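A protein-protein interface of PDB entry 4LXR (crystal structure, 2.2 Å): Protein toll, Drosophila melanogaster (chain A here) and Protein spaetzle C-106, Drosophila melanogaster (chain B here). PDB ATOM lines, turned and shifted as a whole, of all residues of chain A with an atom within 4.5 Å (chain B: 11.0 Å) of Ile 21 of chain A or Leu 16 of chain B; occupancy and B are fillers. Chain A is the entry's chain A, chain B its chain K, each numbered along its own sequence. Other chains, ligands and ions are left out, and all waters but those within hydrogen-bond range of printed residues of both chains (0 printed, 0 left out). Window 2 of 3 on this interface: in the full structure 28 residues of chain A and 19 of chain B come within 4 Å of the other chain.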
ATOM      1  N   ALA A  19     -12.277 -13.635  20.754  1.00  0.00           N
ATOM      2  CA  ALA A  19     -12.615 -13.262  22.119  1.00  0.00           C
ATOM      3  C   ALA A  19     -14.115 -13.054  22.213  1.00  0.00           C
ATOM      4  O   ALA A  19     -14.692 -12.337  21.389  1.00  0.00           O
ATOM      5  CB  ALA A  19     -11.861 -11.996  22.544  1.00  0.00           C
ATOM      6  N   PRO A  20     -14.760 -13.702  23.197  1.00  0.00           N
ATOM      7  CA  PRO A  20     -16.182 -13.438  23.423  1.00  0.00           C
ATOM      8  C   PRO A  20     -16.358 -12.014  23.906  1.00  0.00           C
ATOM      9  O   PRO A  20     -15.483 -11.485  24.579  1.00  0.00           O
ATOM     10  CB  PRO A  20     -16.553 -14.424  24.534  1.00  0.00           C
ATOM     11  CG  PRO A  20     -15.265 -14.720  25.228  1.00  0.00           C
ATOM     12  CD  PRO A  20     -14.231 -14.707  24.132  1.00  0.00           C
ATOM     13  N   ILE A  21     -17.463 -11.388  23.536  1.00  0.00           N
ATOM     14  CA  ILE A  21     -17.775 -10.062  24.040  1.00  0.00           C
ATOM     15  C   ILE A  21     -19.279  -9.839  23.990  1.00  0.00           C
ATOM     16  O   ILE A  21     -19.894  -9.893  22.919  1.00  0.00           O
ATOM     17  CB  ILE A  21     -16.986  -8.939  23.320  1.00  0.00           C
ATOM     18  CG1 ILE A  21     -17.401  -7.578  23.868  1.00  0.00           C
ATOM     19  CG2 ILE A  21     -17.170  -8.990  21.815  1.00  0.00           C
ATOM     20  CD1 ILE A  21     -16.641  -6.438  23.269  1.00  0.00           C
ATOM     21  N   MET A  22     -19.862  -9.600  25.164  1.00  0.00           N
ATOM     22  CA  MET A  22     -21.309  -9.654  25.337  1.00  0.00           C
ATOM     23  C   MET A  22     -21.836 -10.987  24.815  1.00  0.00           C
ATOM     24  O   MET A  22     -21.293 -12.044  25.136  1.00  0.00           O
ATOM     25  CB  MET A  22     -21.996  -8.460  24.672  1.00  0.00           C
ATOM     26  CG  MET A  22     -22.021  -7.226  25.570  1.00  0.00           C
ATOM     27  SD  MET A  22     -21.381  -5.724  24.802  1.00  0.00           S
ATOM     28  CE  MET A  22     -21.379  -4.645  26.229  1.00  0.00           C
ATOM     29  N   SER A  23     -22.880 -10.950  24.002  1.00  0.00           N
ATOM     30  CA  SER A  23     -23.428 -12.192  23.476  1.00  0.00           C
ATOM     31  C   SER A  23     -22.752 -12.620  22.167  1.00  0.00           C
ATOM     32  O   SER A  23     -23.062 -13.677  21.616  1.00  0.00           O
ATOM     33  CB  SER A  23     -24.942 -12.074  23.305  1.00  0.00           C
ATOM     34  OG  SER A  23     -25.287 -10.793  22.811  1.00  0.00           O
ATOM     35  N   GLU A  24     -21.807 -11.820  21.685  1.00  0.00           N
ATOM     36  CA  GLU A  24     -21.166 -12.115  20.406  1.00  0.00           C
ATOM     37  C   GLU A  24     -19.704 -12.547  20.514  1.00  0.00           C
ATOM     38  O   GLU A  24     -19.154 -12.689  21.605  1.00  0.00           O
ATOM     39  CB  GLU A  24     -21.284 -10.912  19.468  1.00  0.00           C
ATOM     40  CG  GLU A  24     -20.440  -9.730  19.894  1.00  0.00           C
ATOM     41  CD  GLU A  24     -20.797  -8.459  19.157  1.00  0.00           C
ATOM     42  OE1 GLU A  24     -20.036  -7.470  19.287  1.00  0.00           O
ATOM     43  OE2 GLU A  24     -21.829  -8.452  18.443  1.00  0.00           O
ATOM     44  N   GLU A  26     -15.795 -11.774  18.613  1.00  0.00           N
ATOM     45  CA  GLU A  26     -15.012 -11.057  17.624  1.00  0.00           C
ATOM     46  C   GLU A  26     -13.814 -11.894  17.211  1.00  0.00           C
ATOM     47  O   GLU A  26     -13.008 -12.293  18.046  1.00  0.00           O
ATOM     48  CB  GLU A  26     -14.543  -9.692  18.124  1.00  0.00           C
ATOM     49  CG  GLU A  26     -13.933  -8.848  17.007  1.00  0.00           C
ATOM     50  CD  GLU A  26     -13.037  -7.728  17.505  1.00  0.00           C
ATOM     51  OE1 GLU A  26     -11.978  -8.020  18.107  1.00  0.00           O
ATOM     52  OE2 GLU A  26     -13.386  -6.552  17.281  1.00  0.00           O
ATOM     53  N   ARG A  39     -12.052  -9.057  10.236  1.00  0.00           N
ATOM     54  CA  ARG A  39     -12.571  -8.952  11.575  1.00  0.00           C
ATOM     55  C   ARG A  39     -13.997  -9.439  11.502  1.00  0.00           C
ATOM     56  O   ARG A  39     -14.833  -8.810  10.868  1.00  0.00           O
ATOM     57  CB  ARG A  39     -12.523  -7.505  12.068  1.00  0.00           C
ATOM     58  CG  ARG A  39     -12.884  -7.353  13.527  1.00  0.00           C
ATOM     59  CD  ARG A  39     -12.882  -5.891  13.957  1.00  0.00           C
ATOM     60  NE  ARG A  39     -11.674  -5.185  13.536  1.00  0.00           N
ATOM     61  CZ  ARG A  39     -10.596  -5.025  14.298  1.00  0.00           C
ATOM     62  NH1 ARG A  39     -10.566  -5.524  15.524  1.00  0.00           N
ATOM     63  NH2 ARG A  39      -9.543  -4.365  13.831  1.00  0.00           N
ATOM     64  N   ILE B  13     -17.155   1.757  12.829  1.00  0.00           N
ATOM     65  CA  ILE B  13     -16.469   0.489  13.019  1.00  0.00           C
ATOM     66  C   ILE B  13     -16.337   0.186  14.504  1.00  0.00           C
ATOM     67  O   ILE B  13     -15.712   0.950  15.237  1.00  0.00           O
ATOM     68  CB  ILE B  13     -15.040   0.566  12.448  1.00  0.00           C
ATOM     69  CG1 ILE B  13     -15.061   1.104  11.014  1.00  0.00           C
ATOM     70  CG2 ILE B  13     -14.349  -0.791  12.535  1.00  0.00           C
ATOM     71  CD1 ILE B  13     -13.686   1.530  10.503  1.00  0.00           C
ATOM     72  N   ARG B  14     -16.922  -0.918  14.961  1.00  0.00           N
ATOM     73  CA  ARG B  14     -16.715  -1.352  16.344  1.00  0.00           C
ATOM     74  C   ARG B  14     -15.531  -2.296  16.392  1.00  0.00           C
ATOM     75  O   ARG B  14     -15.411  -3.173  15.546  1.00  0.00           O
ATOM     76  CB  ARG B  14     -17.958  -2.061  16.897  1.00  0.00           C
ATOM     77  CG  ARG B  14     -19.179  -1.166  17.039  1.00  0.00           C
ATOM     78  CD  ARG B  14     -20.392  -1.924  17.573  1.00  0.00           C
ATOM     79  NE  ARG B  14     -20.238  -2.368  18.958  1.00  0.00           N
ATOM     80  CZ  ARG B  14     -20.466  -1.601  20.023  1.00  0.00           C
ATOM     81  NH1 ARG B  14     -20.843  -0.335  19.875  1.00  0.00           N
ATOM     82  NH2 ARG B  14     -20.307  -2.095  21.242  1.00  0.00           N
ATOM     83  N   LYS B  15     -14.643  -2.125  17.366  1.00  0.00           N
ATOM     84  CA  LYS B  15     -13.536  -3.070  17.515  1.00  0.00           C
ATOM     85  C   LYS B  15     -12.971  -3.156  18.929  1.00  0.00           C
ATOM     86  O   LYS B  15     -13.169  -2.258  19.751  1.00  0.00           O
ATOM     87  CB  LYS B  15     -12.410  -2.770  16.517  1.00  0.00           C
ATOM     88  CG  LYS B  15     -11.658  -1.477  16.756  1.00  0.00           C
ATOM     89  CD  LYS B  15     -10.570  -1.281  15.708  1.00  0.00           C
ATOM     90  CE  LYS B  15      -9.884   0.071  15.850  1.00  0.00           C
ATOM     91  NZ  LYS B  15      -8.839   0.277  14.808  1.00  0.00           N
ATOM     92  N   LEU B  16     -12.271  -4.252  19.204  1.00  0.00           N
ATOM     93  CA  LEU B  16     -11.575  -4.424  20.472  1.00  0.00           C
ATOM     94  C   LEU B  16     -10.184  -3.791  20.429  1.00  0.00           C
ATOM     95  O   LEU B  16      -9.504  -3.841  19.404  1.00  0.00           O
ATOM     96  CB  LEU B  16     -11.444  -5.910  20.808  1.00  0.00           C
ATOM     97  CG  LEU B  16     -12.690  -6.616  21.332  1.00  0.00           C
ATOM     98  CD1 LEU B  16     -12.348  -8.050  21.721  1.00  0.00           C
ATOM     99  CD2 LEU B  16     -13.259  -5.843  22.509  1.00  0.00           C
ATOM    100  N   VAL B  17      -9.764  -3.193  21.542  1.00  0.00           N
ATOM    101  CA  VAL B  17      -8.407  -2.665  21.661  1.00  0.00           C
ATOM    102  C   VAL B  17      -7.785  -3.078  22.990  1.00  0.00           C
ATOM    103  O   VAL B  17      -6.733  -3.721  23.023  1.00  0.00           O
ATOM    104  CB  VAL B  17      -8.364  -1.125  21.537  1.00  0.00           C
ATOM    105  CG1 VAL B  17      -6.928  -0.630  21.610  1.00  0.00           C
ATOM    106  CG2 VAL B  17      -9.004  -0.672  20.241  1.00  0.00           C
ATOM    107  N   GLN B  40      -7.068  -5.400  30.181  1.00  0.00           N
ATOM    108  CA  GLN B  40      -8.229  -6.070  29.602  1.00  0.00           C
ATOM    109  C   GLN B  40      -8.540  -5.564  28.200  1.00  0.00           C
ATOM    110  O   GLN B  40      -7.885  -4.652  27.696  1.00  0.00           O
ATOM    111  CB  GLN B  40      -9.455  -5.905  30.504  1.00  0.00           C
ATOM    112  CG  GLN B  40      -9.406  -6.751  31.766  1.00  0.00           C
ATOM    113  CD  GLN B  40      -9.367  -8.242  31.465  1.00  0.00           C
ATOM    114  OE1 GLN B  40     -10.100  -8.732  30.599  1.00  0.00           O
ATOM    115  NE2 GLN B  40      -8.505  -8.969  32.173  1.00  0.00           N
ATOM    116  N   ALA B  41      -9.547  -6.160  27.572  1.00  0.00           N
ATOM    117  CA  ALA B  41      -9.946  -5.775  26.221  1.00  0.00           C
ATOM    118  C   ALA B  41     -11.015  -4.674  26.225  1.00  0.00           C
ATOM    119  O   ALA B  41     -12.112  -4.857  26.755  1.00  0.00           O
ATOM    120  CB  ALA B  41     -10.432  -6.993  25.450  1.00  0.00           C
ATOM    121  N   ILE B  42     -10.683  -3.533  25.625  1.00  0.00           N
ATOM    122  CA  ILE B  42     -11.591  -2.390  25.554  1.00  0.00           C
ATOM    123  C   ILE B  42     -12.169  -2.235  24.146  1.00  0.00           C
ATOM    124  O   ILE B  42     -11.426  -2.194  23.164  1.00  0.00           O
ATOM    125  CB  ILE B  42     -10.859  -1.091  25.960  1.00  0.00           C
ATOM    126  CG1 ILE B  42     -11.645   0.151  25.525  1.00  0.00           C
ATOM    127  CG2 ILE B  42      -9.456  -1.070  25.366  1.00  0.00           C
ATOM    128  CD1 ILE B  42     -12.919   0.396  26.311  1.00  0.00           C
ATOM    129  N   GLN B  43     -13.492  -2.157  24.039  1.00  0.00           N
ATOM    130  CA  GLN B  43     -14.096  -1.962  22.733  1.00  0.00           C
ATOM    131  C   GLN B  43     -14.478  -0.509  22.476  1.00  0.00           C
ATOM    132  O   GLN B  43     -14.934   0.210  23.369  1.00  0.00           O
ATOM    133  CB  GLN B  43     -15.281  -2.903  22.503  1.00  0.00           C
ATOM    134  CG  GLN B  43     -16.588  -2.475  23.123  1.00  0.00           C
ATOM    135  CD  GLN B  43     -17.749  -3.323  22.635  1.00  0.00           C
ATOM    136  OE1 GLN B  43     -17.705  -3.889  21.534  1.00  0.00           O
ATOM    137  NE2 GLN B  43     -18.790  -3.429  23.458  1.00  0.00           N
ATOM    138  N   ILE B  44     -14.264  -0.079  21.241  1.00  0.00           N
ATOM    139  CA  ILE B  44     -14.479   1.303  20.869  1.00  0.00           C
ATOM    140  C   ILE B  44     -15.340   1.366  19.623  1.00  0.00           C
ATOM    141  O   ILE B  44     -15.433   0.393  18.878  1.00  0.00           O
ATOM    142  CB  ILE B  44     -13.142   2.009  20.590  1.00  0.00           C
ATOM    143  CG1 ILE B  44     -12.497   1.445  19.320  1.00  0.00           C
ATOM    144  CG2 ILE B  44     -12.214   1.856  21.772  1.00  0.00           C
ATOM    145  CD1 ILE B  44     -11.143   2.044  19.005  1.00  0.00           C
ATOM    146  N   GLU B  45     -15.989   2.505  19.413  1.00  0.00           N
ATOM    147  CA  GLU B  45     -16.685   2.756  18.159  1.00  0.00           C
ATOM    148  C   GLU B  45     -16.201   4.062  17.556  1.00  0.00           C
ATOM    149  O   GLU B  45     -16.249   5.104  18.213  1.00  0.00           O
ATOM    150  CB  GLU B  45     -18.198   2.799  18.364  1.00  0.00           C
ATOM    151  CG  GLU B  45     -18.981   2.969  17.056  1.00  0.00           C
ATOM    152  CD  GLU B  45     -20.473   2.805  17.250  1.00  0.00           C
ATOM    153  OE1 GLU B  45     -21.240   3.749  16.931  1.00  0.00           O
ATOM    154  OE2 GLU B  45     -20.868   1.723  17.735  1.00  0.00           O
ATOM    155  N   GLU B  46     -15.723   4.000  16.316  1.00  0.00           N
ATOM    156  CA  GLU B  46     -15.199   5.181  15.629  1.00  0.00           C
ATOM    157  C   GLU B  46     -15.970   5.455  14.362  1.00  0.00           C
ATOM    158  O   GLU B  46     -16.367   4.520  13.679  1.00  0.00           O
ATOM    159  CB  GLU B  46     -13.733   4.989  15.248  1.00  0.00           C
ATOM    160  CG  GLU B  46     -12.761   5.080  16.396  1.00  0.00           C
ATOM    161  CD  GLU B  46     -11.325   4.970  15.934  1.00  0.00           C
ATOM    162  OE1 GLU B  46     -11.029   4.048  15.146  1.00  0.00           O
ATOM    163  OE2 GLU B  46     -10.496   5.812  16.355  1.00  0.00           O
ATOM    164  N   ILE B  95     -12.259   7.664  25.298  1.00  0.00           N
ATOM    165  CA  ILE B  95     -12.467   6.480  24.468  1.00  0.00           C
ATOM    166  C   ILE B  95     -13.571   6.765  23.446  1.00  0.00           C
ATOM    167  O   ILE B  95     -14.681   7.121  23.832  1.00  0.00           O
ATOM    168  CB  ILE B  95     -12.895   5.265  25.334  1.00  0.00           C
ATOM    169  CG1 ILE B  95     -11.830   4.939  26.382  1.00  0.00           C
ATOM    170  CG2 ILE B  95     -13.162   4.049  24.473  1.00  0.00           C
ATOM    171  CD1 ILE B  95     -10.535   4.413  25.800  1.00  0.00           C
ATOM    172  N   PRO B  96     -13.268   6.627  22.141  1.00  0.00           N
ATOM    173  CA  PRO B  96     -14.324   6.759  21.123  1.00  0.00           C
ATOM    174  C   PRO B  96     -15.432   5.763  21.440  1.00  0.00           C
ATOM    175  O   PRO B  96     -15.134   4.575  21.576  1.00  0.00           O
ATOM    176  CB  PRO B  96     -13.612   6.375  19.826  1.00  0.00           C
ATOM    177  CG  PRO B  96     -12.168   6.631  20.095  1.00  0.00           C
ATOM    178  CD  PRO B  96     -11.960   6.308  21.544  1.00  0.00           C
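The side-chain sulfur of Met 22 of chain A sits at hydrogen-bond distance from the side-chain amide nitrogen of Gln 43 of chain B, 3.7 Å away.
N of Leu 16 of chain B lies within hydrogen-bond range of OE2 of Glu 26 of chain A (3.2 Å).
Printed residues of chain B that touch a printed residue of chain A: Lys 15, Leu 16 and Gln 43.
Hydrophobic or aromatic side chains of chain B within 4 Å of the printed part of chain A: Leu 16.
Of the 8 printed residues of chain A, 4 touch a printed residue of chain B.
Hydrophobic or aromatic side chains of chain A within 4 Å of the printed part of chain B: Ile 21 and Met 22.
Among the printed residues, 6 pairs touch across the chains.
Among the printed residues, no Asp or Glu carboxylate lies within 4 Å of a Lys or Arg side-chain nitrogen of the other chain.
No residue of chain B comes within 4 Å of Ala 19 of chain A.
No residue of chain B comes within 4 Å of Pro 20 of chain A.
Ile 21 of chain A touches two residues of chain B.
Met 22 of chain A touches just one residue of chain B: Gln 43 (3.7 Å).
No residue of chain B comes within 4 Å of Ser 23 of chain A.
Glu 24 of chain A touches none of the printed residues of chain B.
Printed residues of chain B within 4 Å of Arg 39 of chain A: Lys 15.
Of the printed residues of chain A, Lys 15 of chain B touches Glu 26 (3.5 Å) and Arg 39 (3.5 Å).
Of chain A, only Ile 21 (3.5 Å) and Glu 26 (3.2 Å) come within 4 Å of Leu 16 of chain B.
Of the printed residues of chain A, Gln 43 of chain B touches Ile 21 and Met 22.
The nearest residue of chain A that does not touch Leu 16 of chain B is Ala 19 of chain A (4.1 Å).
The nearest printed residue of chain A that does not touch Lys 15 of chain B is Ile 21 of chain A (6.5 Å).
Among the printed residues, merely in contact across the chains: Ile 21 of chain A with Leu 16 of chain B, Ile 21 of chain A with Gln 43 of chain B, Glu 26 of chain A with Lys 15 of chain B and Arg 39 of chain A with Lys 15 of chain B.
The backbone NH (N) of Glu 26 of chain A is in hydrogen-bond range of the backbone carbonyl oxygen (O) of Ala 19 of chain A (3.0 Å).
OE2 of Glu 26 of chain A lies within salt-bridge range of NH1 of Arg 39 of chain A.
The side-chain amide nitrogen of Gln 43 of chain B sits close to the guanidinium group of Arg 14 of chain B (3.0 Å).
The backbone carbonyl oxygen of Lys 15 of chain B lies within hydrogen-bond range of the backbone NH of Ile 44 of chain B (2.9 Å).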
